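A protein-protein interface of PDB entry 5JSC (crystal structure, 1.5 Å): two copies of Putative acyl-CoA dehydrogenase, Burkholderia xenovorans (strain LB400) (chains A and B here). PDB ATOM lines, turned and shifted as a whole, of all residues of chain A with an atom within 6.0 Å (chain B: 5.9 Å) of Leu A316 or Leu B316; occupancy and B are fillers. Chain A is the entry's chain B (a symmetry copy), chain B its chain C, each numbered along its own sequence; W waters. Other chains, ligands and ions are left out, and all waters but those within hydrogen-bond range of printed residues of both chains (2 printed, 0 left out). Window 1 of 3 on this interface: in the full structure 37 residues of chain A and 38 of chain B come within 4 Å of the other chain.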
ATOM      1  N   TRP A  23      27.656  -4.946  28.205  1.00  0.00           N
ATOM      2  CA  TRP A  23      27.867  -5.924  29.263  1.00  0.00           C
ATOM      3  C   TRP A  23      29.170  -5.644  30.002  1.00  0.00           C
ATOM      4  O   TRP A  23      30.165  -5.245  29.380  1.00  0.00           O
ATOM      5  CB  TRP A  23      27.934  -7.341  28.700  1.00  0.00           C
ATOM      6  CG  TRP A  23      26.690  -7.822  28.044  1.00  0.00           C
ATOM      7  CD1 TRP A  23      25.425  -7.336  28.202  1.00  0.00           C
ATOM      8  CD2 TRP A  23      26.600  -8.900  27.116  1.00  0.00           C
ATOM      9  NE1 TRP A  23      24.544  -8.058  27.423  1.00  0.00           N
ATOM     10  CE2 TRP A  23      25.247  -9.022  26.745  1.00  0.00           C
ATOM     11  CE3 TRP A  23      27.538  -9.771  26.554  1.00  0.00           C
ATOM     12  CZ2 TRP A  23      24.810  -9.979  25.836  1.00  0.00           C
ATOM     13  CZ3 TRP A  23      27.104 -10.726  25.655  1.00  0.00           C
ATOM     14  CH2 TRP A  23      25.753 -10.821  25.302  1.00  0.00           C
ATOM     15  N   PHE A  25      31.332  -7.614  30.962  1.00  0.00           N
ATOM     16  CA  PHE A  25      32.435  -8.406  30.433  1.00  0.00           C
ATOM     17  C   PHE A  25      33.393  -7.568  29.600  1.00  0.00           C
ATOM     18  O   PHE A  25      34.519  -8.009  29.346  1.00  0.00           O
ATOM     19  CB  PHE A  25      31.908  -9.548  29.557  1.00  0.00           C
ATOM     20  CG  PHE A  25      31.209 -10.656  30.315  1.00  0.00           C
ATOM     21  CD1 PHE A  25      31.826 -11.303  31.377  1.00  0.00           C
ATOM     22  CD2 PHE A  25      29.940 -11.071  29.934  1.00  0.00           C
ATOM     23  CE1 PHE A  25      31.188 -12.331  32.056  1.00  0.00           C
ATOM     24  CE2 PHE A  25      29.286 -12.100  30.614  1.00  0.00           C
ATOM     25  CZ  PHE A  25      29.914 -12.734  31.671  1.00  0.00           C
ATOM     26  N   ILE A 311      21.550 -16.656  19.612  1.00  0.00           N
ATOM     27  CA  ILE A 311      22.623 -15.673  19.462  1.00  0.00           C
ATOM     28  C   ILE A 311      23.005 -15.075  20.815  1.00  0.00           C
ATOM     29  O   ILE A 311      24.195 -14.964  21.141  1.00  0.00           O
ATOM     30  CB  ILE A 311      22.210 -14.596  18.444  1.00  0.00           C
ATOM     31  CG1 ILE A 311      22.350 -15.179  17.043  1.00  0.00           C
ATOM     32  CG2 ILE A 311      23.045 -13.315  18.599  1.00  0.00           C
ATOM     33  CD1 ILE A 311      21.703 -14.345  15.971  1.00  0.00           C
ATOM     34  N   ASP A 312      22.019 -14.695  21.635  1.00  0.00           N
ATOM     35  CA  ASP A 312      22.374 -14.088  22.925  1.00  0.00           C
ATOM     36  C   ASP A 312      23.064 -15.095  23.837  1.00  0.00           C
ATOM     37  O   ASP A 312      24.044 -14.756  24.517  1.00  0.00           O
ATOM     38  CB  ASP A 312      21.145 -13.500  23.631  1.00  0.00           C
ATOM     39  CG  ASP A 312      20.803 -12.093  23.159  1.00  0.00           C
ATOM     40  OD1 ASP A 312      21.382 -11.637  22.149  1.00  0.00           O
ATOM     41  OD2 ASP A 312      19.933 -11.447  23.792  1.00  0.00           O
ATOM     42  N   SER A 313      22.577 -16.338  23.877  1.00  0.00           N
ATOM     43  CA  SER A 313      23.250 -17.321  24.714  1.00  0.00           C
ATOM     44  C   SER A 313      24.662 -17.599  24.206  1.00  0.00           C
ATOM     45  O   SER A 313      25.600 -17.691  25.011  1.00  0.00           O
ATOM     46  CB  SER A 313      22.421 -18.601  24.804  1.00  0.00           C
ATOM     47  OG  SER A 313      22.140 -19.117  23.526  1.00  0.00           O
ATOM     48  N   SER A 314      24.843 -17.707  22.885  1.00  0.00           N
ATOM     49  CA  SER A 314      26.186 -17.886  22.333  1.00  0.00           C
ATOM     50  C   SER A 314      27.090 -16.719  22.689  1.00  0.00           C
ATOM     51  O   SER A 314      28.240 -16.916  23.096  1.00  0.00           O
ATOM     52  CB  SER A 314      26.130 -18.042  20.811  1.00  0.00           C
ATOM     53  OG  SER A 314      25.455 -19.230  20.435  1.00  0.00           O
ATOM     54  N   ALA A 315      26.593 -15.490  22.517  1.00  0.00           N
ATOM     55  CA  ALA A 315      27.413 -14.315  22.797  1.00  0.00           C
ATOM     56  C   ALA A 315      27.812 -14.267  24.263  1.00  0.00           C
ATOM     57  O   ALA A 315      28.971 -13.972  24.589  1.00  0.00           O
ATOM     58  CB  ALA A 315      26.666 -13.036  22.406  1.00  0.00           C
ATOM     59  N   LEU A 316      26.869 -14.557  25.163  1.00  0.00           N
ATOM     60  CA  LEU A 316      27.197 -14.577  26.587  1.00  0.00           C
ATOM     61  C   LEU A 316      28.249 -15.635  26.900  1.00  0.00           C
ATOM     62  O   LEU A 316      29.177 -15.379  27.676  1.00  0.00           O
ATOM     63  CB  LEU A 316      25.925 -14.793  27.418  1.00  0.00           C
ATOM     64  CG  LEU A 316      25.025 -13.552  27.477  1.00  0.00           C
ATOM     65  CD1 LEU A 316      23.601 -13.952  27.818  1.00  0.00           C
ATOM     66  CD2 LEU A 316      25.551 -12.533  28.497  1.00  0.00           C
ATOM     67  N   LEU A 317      28.142 -16.819  26.288  1.00  0.00           N
ATOM     68  CA  LEU A 317      29.140 -17.861  26.531  1.00  0.00           C
ATOM     69  C   LEU A 317      30.504 -17.475  25.964  1.00  0.00           C
ATOM     70  O   LEU A 317      31.534 -17.717  26.607  1.00  0.00           O
ATOM     71  CB  LEU A 317      28.674 -19.189  25.931  1.00  0.00           C
ATOM     72  CG  LEU A 317      27.495 -19.867  26.629  1.00  0.00           C
ATOM     73  CD1 LEU A 317      26.869 -20.897  25.697  1.00  0.00           C
ATOM     74  CD2 LEU A 317      27.940 -20.499  27.942  1.00  0.00           C
ATOM     75  N   VAL A 318      30.533 -16.886  24.763  1.00  0.00           N
ATOM     76  CA  VAL A 318      31.798 -16.455  24.163  1.00  0.00           C
ATOM     77  C   VAL A 318      32.500 -15.463  25.073  1.00  0.00           C
ATOM     78  O   VAL A 318      33.681 -15.624  25.407  1.00  0.00           O
ATOM     79  CB  VAL A 318      31.562 -15.848  22.765  1.00  0.00           C
ATOM     80  CG1 VAL A 318      32.830 -15.139  22.259  1.00  0.00           C
ATOM     81  CG2 VAL A 318      31.098 -16.921  21.763  1.00  0.00           C
ATOM     82  N   TYR A 319      31.793 -14.408  25.470  1.00  0.00           N
ATOM     83  CA  TYR A 319      32.486 -13.337  26.170  1.00  0.00           C
ATOM     84  C   TYR A 319      32.640 -13.610  27.662  1.00  0.00           C
ATOM     85  O   TYR A 319      33.553 -13.046  28.277  1.00  0.00           O
ATOM     86  CB  TYR A 319      31.804 -11.994  25.858  1.00  0.00           C
ATOM     87  CG  TYR A 319      32.082 -11.684  24.408  1.00  0.00           C
ATOM     88  CD1 TYR A 319      33.350 -11.270  24.009  1.00  0.00           C
ATOM     89  CD2 TYR A 319      31.129 -11.913  23.420  1.00  0.00           C
ATOM     90  CE1 TYR A 319      33.650 -11.040  22.679  1.00  0.00           C
ATOM     91  CE2 TYR A 319      31.429 -11.699  22.080  1.00  0.00           C
ATOM     92  CZ  TYR A 319      32.690 -11.260  21.716  1.00  0.00           C
ATOM     93  OH  TYR A 319      33.000 -11.039  20.391  1.00  0.00           O
ATOM     94  N   ARG A 320      31.843 -14.511  28.244  1.00  0.00           N
ATOM     95  CA  ARG A 320      32.198 -15.011  29.568  1.00  0.00           C
ATOM     96  C   ARG A 320      33.552 -15.705  29.515  1.00  0.00           C
ATOM     97  O   ARG A 320      34.424 -15.470  30.363  1.00  0.00           O
ATOM     98  CB  ARG A 320      31.122 -15.969  30.096  1.00  0.00           C
ATOM     99  CG  ARG A 320      31.394 -16.544  31.505  1.00  0.00           C
ATOM    100  CD  ARG A 320      32.268 -17.817  31.519  1.00  0.00           C
ATOM    101  NE  ARG A 320      31.655 -18.941  30.797  1.00  0.00           N
ATOM    102  CZ  ARG A 320      30.926 -19.906  31.367  1.00  0.00           C
ATOM    103  NH1 ARG A 320      30.709 -19.917  32.679  1.00  0.00           N
ATOM    104  NH2 ARG A 320      30.400 -20.868  30.621  1.00  0.00           N
ATOM    105  N   ALA A 321      33.736 -16.587  28.529  1.00  0.00           N
ATOM    106  CA  ALA A 321      34.989 -17.322  28.424  1.00  0.00           C
ATOM    107  C   ALA A 321      36.156 -16.388  28.133  1.00  0.00           C
ATOM    108  O   ALA A 321      37.235 -16.537  28.717  1.00  0.00           O
ATOM    109  CB  ALA A 321      34.873 -18.399  27.346  1.00  0.00           C
ATOM    110  N   TRP B  23      31.343 -13.419  38.004  1.00  0.00           N
ATOM    111  CA  TRP B  23      31.020 -12.647  36.813  1.00  0.00           C
ATOM    112  C   TRP B  23      30.847 -11.174  37.164  1.00  0.00           C
ATOM    113  O   TRP B  23      30.304 -10.846  38.230  1.00  0.00           O
ATOM    114  CB  TRP B  23      29.727 -13.136  36.154  1.00  0.00           C
ATOM    115  CG  TRP B  23      29.767 -14.533  35.654  1.00  0.00           C
ATOM    116  CD1 TRP B  23      30.872 -15.291  35.402  1.00  0.00           C
ATOM    117  CD2 TRP B  23      28.634 -15.344  35.341  1.00  0.00           C
ATOM    118  NE1 TRP B  23      30.492 -16.536  34.946  1.00  0.00           N
ATOM    119  CE2 TRP B  23      29.121 -16.594  34.910  1.00  0.00           C
ATOM    120  CE3 TRP B  23      27.252 -15.141  35.410  1.00  0.00           C
ATOM    121  CZ2 TRP B  23      28.272 -17.639  34.528  1.00  0.00           C
ATOM    122  CZ3 TRP B  23      26.408 -16.175  35.031  1.00  0.00           C
ATOM    123  CH2 TRP B  23      26.920 -17.410  34.601  1.00  0.00           C
ATOM    124  N   PHE B  25      28.724  -9.175  36.181  1.00  0.00           N
ATOM    125  CA  PHE B  25      27.331  -8.839  36.438  1.00  0.00           C
ATOM    126  C   PHE B  25      27.062  -8.622  37.920  1.00  0.00           C
ATOM    127  O   PHE B  25      26.071  -7.971  38.262  1.00  0.00           O
ATOM    128  CB  PHE B  25      26.396  -9.953  35.952  1.00  0.00           C
ATOM    129  CG  PHE B  25      26.284 -10.082  34.461  1.00  0.00           C
ATOM    130  CD1 PHE B  25      26.008  -8.986  33.667  1.00  0.00           C
ATOM    131  CD2 PHE B  25      26.412 -11.325  33.856  1.00  0.00           C
ATOM    132  CE1 PHE B  25      25.872  -9.118  32.291  1.00  0.00           C
ATOM    133  CE2 PHE B  25      26.286 -11.464  32.480  1.00  0.00           C
ATOM    134  CZ  PHE B  25      26.019 -10.359  31.697  1.00  0.00           C
ATOM    135  N   ILE B 311      22.776 -25.092  31.865  1.00  0.00           N
ATOM    136  CA  ILE B 311      22.813 -24.325  33.109  1.00  0.00           C
ATOM    137  C   ILE B 311      23.590 -23.027  32.928  1.00  0.00           C
ATOM    138  O   ILE B 311      23.150 -21.959  33.383  1.00  0.00           O
ATOM    139  CB  ILE B 311      23.384 -25.189  34.247  1.00  0.00           C
ATOM    140  CG1 ILE B 311      22.296 -26.147  34.737  1.00  0.00           C
ATOM    141  CG2 ILE B 311      23.920 -24.310  35.408  1.00  0.00           C
ATOM    142  CD1 ILE B 311      22.815 -27.265  35.610  1.00  0.00           C
ATOM    143  N   ASP B 312      24.749 -23.083  32.268  1.00  0.00           N
ATOM    144  CA  ASP B 312      25.533 -21.853  32.124  1.00  0.00           C
ATOM    145  C   ASP B 312      24.848 -20.863  31.193  1.00  0.00           C
ATOM    146  O   ASP B 312      24.837 -19.659  31.467  1.00  0.00           O
ATOM    147  CB  ASP B 312      26.951 -22.165  31.641  1.00  0.00           C
ATOM    148  CG  ASP B 312      27.885 -22.508  32.783  1.00  0.00           C
ATOM    149  OD1 ASP B 312      27.384 -22.781  33.904  1.00  0.00           O
ATOM    150  OD2 ASP B 312      29.117 -22.512  32.563  1.00  0.00           O
ATOM    151  N   SER B 313      24.256 -21.335  30.093  1.00  0.00           N
ATOM    152  CA  SER B 313      23.553 -20.395  29.228  1.00  0.00           C
ATOM    153  C   SER B 313      22.341 -19.812  29.946  1.00  0.00           C
ATOM    154  O   SER B 313      22.072 -18.610  29.822  1.00  0.00           O
ATOM    155  CB  SER B 313      23.161 -21.057  27.902  1.00  0.00           C
ATOM    156  OG  SER B 313      22.387 -22.218  28.092  1.00  0.00           O
ATOM    157  N   SER B 314      21.626 -20.629  30.729  1.00  0.00           N
ATOM    158  CA  SER B 314      20.508 -20.111  31.516  1.00  0.00           C
ATOM    159  C   SER B 314      20.988 -19.072  32.519  1.00  0.00           C
ATOM    160  O   SER B 314      20.409 -17.986  32.632  1.00  0.00           O
ATOM    161  CB  SER B 314      19.789 -21.245  32.243  1.00  0.00           C
ATOM    162  OG  SER B 314      19.174 -22.128  31.322  1.00  0.00           O
ATOM    163  N   ALA B 315      22.052 -19.392  33.258  1.00  0.00           N
ATOM    164  CA  ALA B 315      22.534 -18.471  34.279  1.00  0.00           C
ATOM    165  C   ALA B 315      22.985 -17.149  33.669  1.00  0.00           C
ATOM    166  O   ALA B 315      22.697 -16.077  34.218  1.00  0.00           O
ATOM    167  CB  ALA B 315      23.672 -19.118  35.068  1.00  0.00           C
ATOM    168  N   LEU B 316      23.702 -17.204  32.543  1.00  0.00           N
ATOM    169  CA  LEU B 316      24.126 -15.978  31.874  1.00  0.00           C
ATOM    170  C   LEU B 316      22.926 -15.146  31.437  1.00  0.00           C
ATOM    171  O   LEU B 316      22.919 -13.920  31.612  1.00  0.00           O
ATOM    172  CB  LEU B 316      25.027 -16.316  30.685  1.00  0.00           C
ATOM    173  CG  LEU B 316      26.444 -16.760  31.104  1.00  0.00           C
ATOM    174  CD1 LEU B 316      27.148 -17.554  29.988  1.00  0.00           C
ATOM    175  CD2 LEU B 316      27.287 -15.542  31.521  1.00  0.00           C
ATOM    176  N   LEU B 317      21.888 -15.795  30.884  1.00  0.00           N
ATOM    177  CA  LEU B 317      20.688 -15.051  30.494  1.00  0.00           C
ATOM    178  C   LEU B 317      19.958 -14.468  31.700  1.00  0.00           C
ATOM    179  O   LEU B 317      19.460 -13.333  31.634  1.00  0.00           O
ATOM    180  CB  LEU B 317      19.752 -15.948  29.691  1.00  0.00           C
ATOM    181  CG  LEU B 317      20.235 -16.313  28.292  1.00  0.00           C
ATOM    182  CD1 LEU B 317      19.383 -17.465  27.770  1.00  0.00           C
ATOM    183  CD2 LEU B 317      20.126 -15.125  27.359  1.00  0.00           C
ATOM    184  N   VAL B 318      19.861 -15.229  32.799  1.00  0.00           N
ATOM    185  CA  VAL B 318      19.211 -14.727  34.011  1.00  0.00           C
ATOM    186  C   VAL B 318      19.904 -13.467  34.497  1.00  0.00           C
ATOM    187  O   VAL B 318      19.265 -12.431  34.726  1.00  0.00           O
ATOM    188  CB  VAL B 318      19.211 -15.802  35.114  1.00  0.00           C
ATOM    189  CG1 VAL B 318      18.812 -15.189  36.462  1.00  0.00           C
ATOM    190  CG2 VAL B 318      18.280 -16.943  34.748  1.00  0.00           C
ATOM    191  N   TYR B 319      21.223 -13.534  34.667  1.00  0.00           N
ATOM    192  CA  TYR B 319      21.905 -12.423  35.312  1.00  0.00           C
ATOM    193  C   TYR B 319      22.257 -11.308  34.339  1.00  0.00           C
ATOM    194  O   TYR B 319      22.418 -10.169  34.780  1.00  0.00           O
ATOM    195  CB  TYR B 319      23.103 -12.962  36.111  1.00  0.00           C
ATOM    196  CG  TYR B 319      22.529 -13.750  37.272  1.00  0.00           C
ATOM    197  CD1 TYR B 319      21.917 -13.091  38.338  1.00  0.00           C
ATOM    198  CD2 TYR B 319      22.502 -15.146  37.267  1.00  0.00           C
ATOM    199  CE1 TYR B 319      21.329 -13.795  39.383  1.00  0.00           C
ATOM    200  CE2 TYR B 319      21.911 -15.854  38.307  1.00  0.00           C
ATOM    201  CZ  TYR B 319      21.323 -15.172  39.367  1.00  0.00           C
ATOM    202  OH  TYR B 319      20.722 -15.848  40.402  1.00  0.00           O
ATOM    203  N   ARG B 320      22.278 -11.570  33.027  1.00  0.00           N
ATOM    204  CA  ARG B 320      22.270 -10.461  32.077  1.00  0.00           C
ATOM    205  C   ARG B 320      21.000  -9.641  32.238  1.00  0.00           C
ATOM    206  O   ARG B 320      21.050  -8.412  32.333  1.00  0.00           O
ATOM    207  CB  ARG B 320      22.402 -10.976  30.636  1.00  0.00           C
ATOM    208  CG  ARG B 320      22.464  -9.878  29.557  1.00  0.00           C
ATOM    209  CD  ARG B 320      21.081  -9.369  29.112  1.00  0.00           C
ATOM    210  NE  ARG B 320      20.290 -10.417  28.463  1.00  0.00           N
ATOM    211  CZ  ARG B 320      20.284 -10.638  27.151  1.00  0.00           C
ATOM    212  NH1 ARG B 320      21.006  -9.883  26.337  1.00  0.00           N
ATOM    213  NH2 ARG B 320      19.548 -11.623  26.648  1.00  0.00           N
ATOM    214  N   ALA B 321      19.846 -10.313  32.273  1.00  0.00           N
ATOM    215  CA  ALA B 321      18.584  -9.594  32.430  1.00  0.00           C
ATOM    216  C   ALA B 321      18.512  -8.879  33.773  1.00  0.00           C
ATOM    217  O   ALA B 321      18.064  -7.726  33.845  1.00  0.00           O
ATOM    218  CB  ALA B 321      17.400 -10.553  32.274  1.00  0.00           C
HETATM  219  O   HOH W   1      21.795  -7.101  26.731  1.00  0.00           O
HETATM  220  O   HOH W   2      32.416 -18.790  34.750  1.00  0.00           O
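The side-chain carboxylate of Asp B312 lies within salt-bridge range of the guanidinium group of Arg A320 (2.8 Å).
The side-chain carboxylate of Asp A312 lies within salt-bridge range of the guanidinium group of Arg B320.
Among the printed residues, merely in contact across the chains: Trp A23 with Arg B320 (3.5 Å), Arg A320 with Trp B23 (3.6 Å), Phe A25 with Phe B25 (3.6 Å), Leu A317 with Leu B316 (3.7 Å), Leu A316 with Leu B317 (3.7 Å), Leu A316 with Leu B316 (3.7 Å), Phe A25 with Leu B316 (3.8 Å) and Leu A316 with Phe B25 (3.9 Å).
Of the printed residues of chain B, Phe A25 touches Phe B25 and Leu B316.
Of chain B, only Phe B25 (3.9 Å), Leu B316 (3.7 Å) and Leu B317 (3.7 Å) come within 4 Å of Leu A316.
Tyr A319 touches none of the printed residues of chain B.
Of the printed residues of chain B, Arg A320 touches Trp B23 and Asp B312.
Of the printed residues of chain A, Phe B25 touches Phe A25 and Leu A316.
Printed residues of chain A within 4 Å of Asp B312: Arg A320 (2.8 Å).
Printed residues of chain A within 4 Å of Leu B317: Leu A316.
The nearest residue of chain B that does not touch Leu A316 is Arg B320 (4.1 Å).
The nearest printed residue of chain B that does not touch Phe A25 is Trp B23 (4.4 Å).
Of the 13 printed residues of chain A, 6 touch a printed residue of chain B.
Printed residues of chain A that touch a printed residue of chain B: Trp A23, Phe A25, Asp A312, Leu A316, Leu A317 and Arg A320.
Hydrophobic or aromatic side chains of chain A that line the printed part of chain B: Trp A23, Phe A25, Leu A316 and Leu A317.
Printed residues of chain B that touch a printed residue of chain A: Trp B23, Phe B25, Asp B312, Leu B316, Leu B317 and Arg B320.
Hydrophobic or aromatic side chains of chain B that line the printed part of chain A: Trp B23, Phe B25, Leu B316 and Leu B317.
Among the printed residues, 10 pairs touch across the chains.
Among the printed residues, Asp or Glu carboxylates within 4 Å of a Lys or Arg side-chain nitrogen of the other chain: Asp A312 with Arg B320 and Arg A320 with Asp B312.
Trp A23 touches Arg B320, and with the chains exchanged Arg A320 touches Trp B23.
Phe B25 touches its own counterpart, Phe A25.
Phe A25 touches Leu B316, and with the chains exchanged Leu A316 touches Phe B25.
Asp A312 touches Arg B320, and with the chains exchanged Arg A320 touches Asp B312.
13 positions are printed for both chains.
Water W2 lies within hydrogen-bond range of NH1 of Arg A320 (2.9 Å) and NE1 of Trp B23 (3.0 Å).
Water W1 lies within hydrogen-bond range of the guanidinium group of Arg B320 (2.9 Å) and the indole nitrogen of Trp A23 (3.0 Å).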
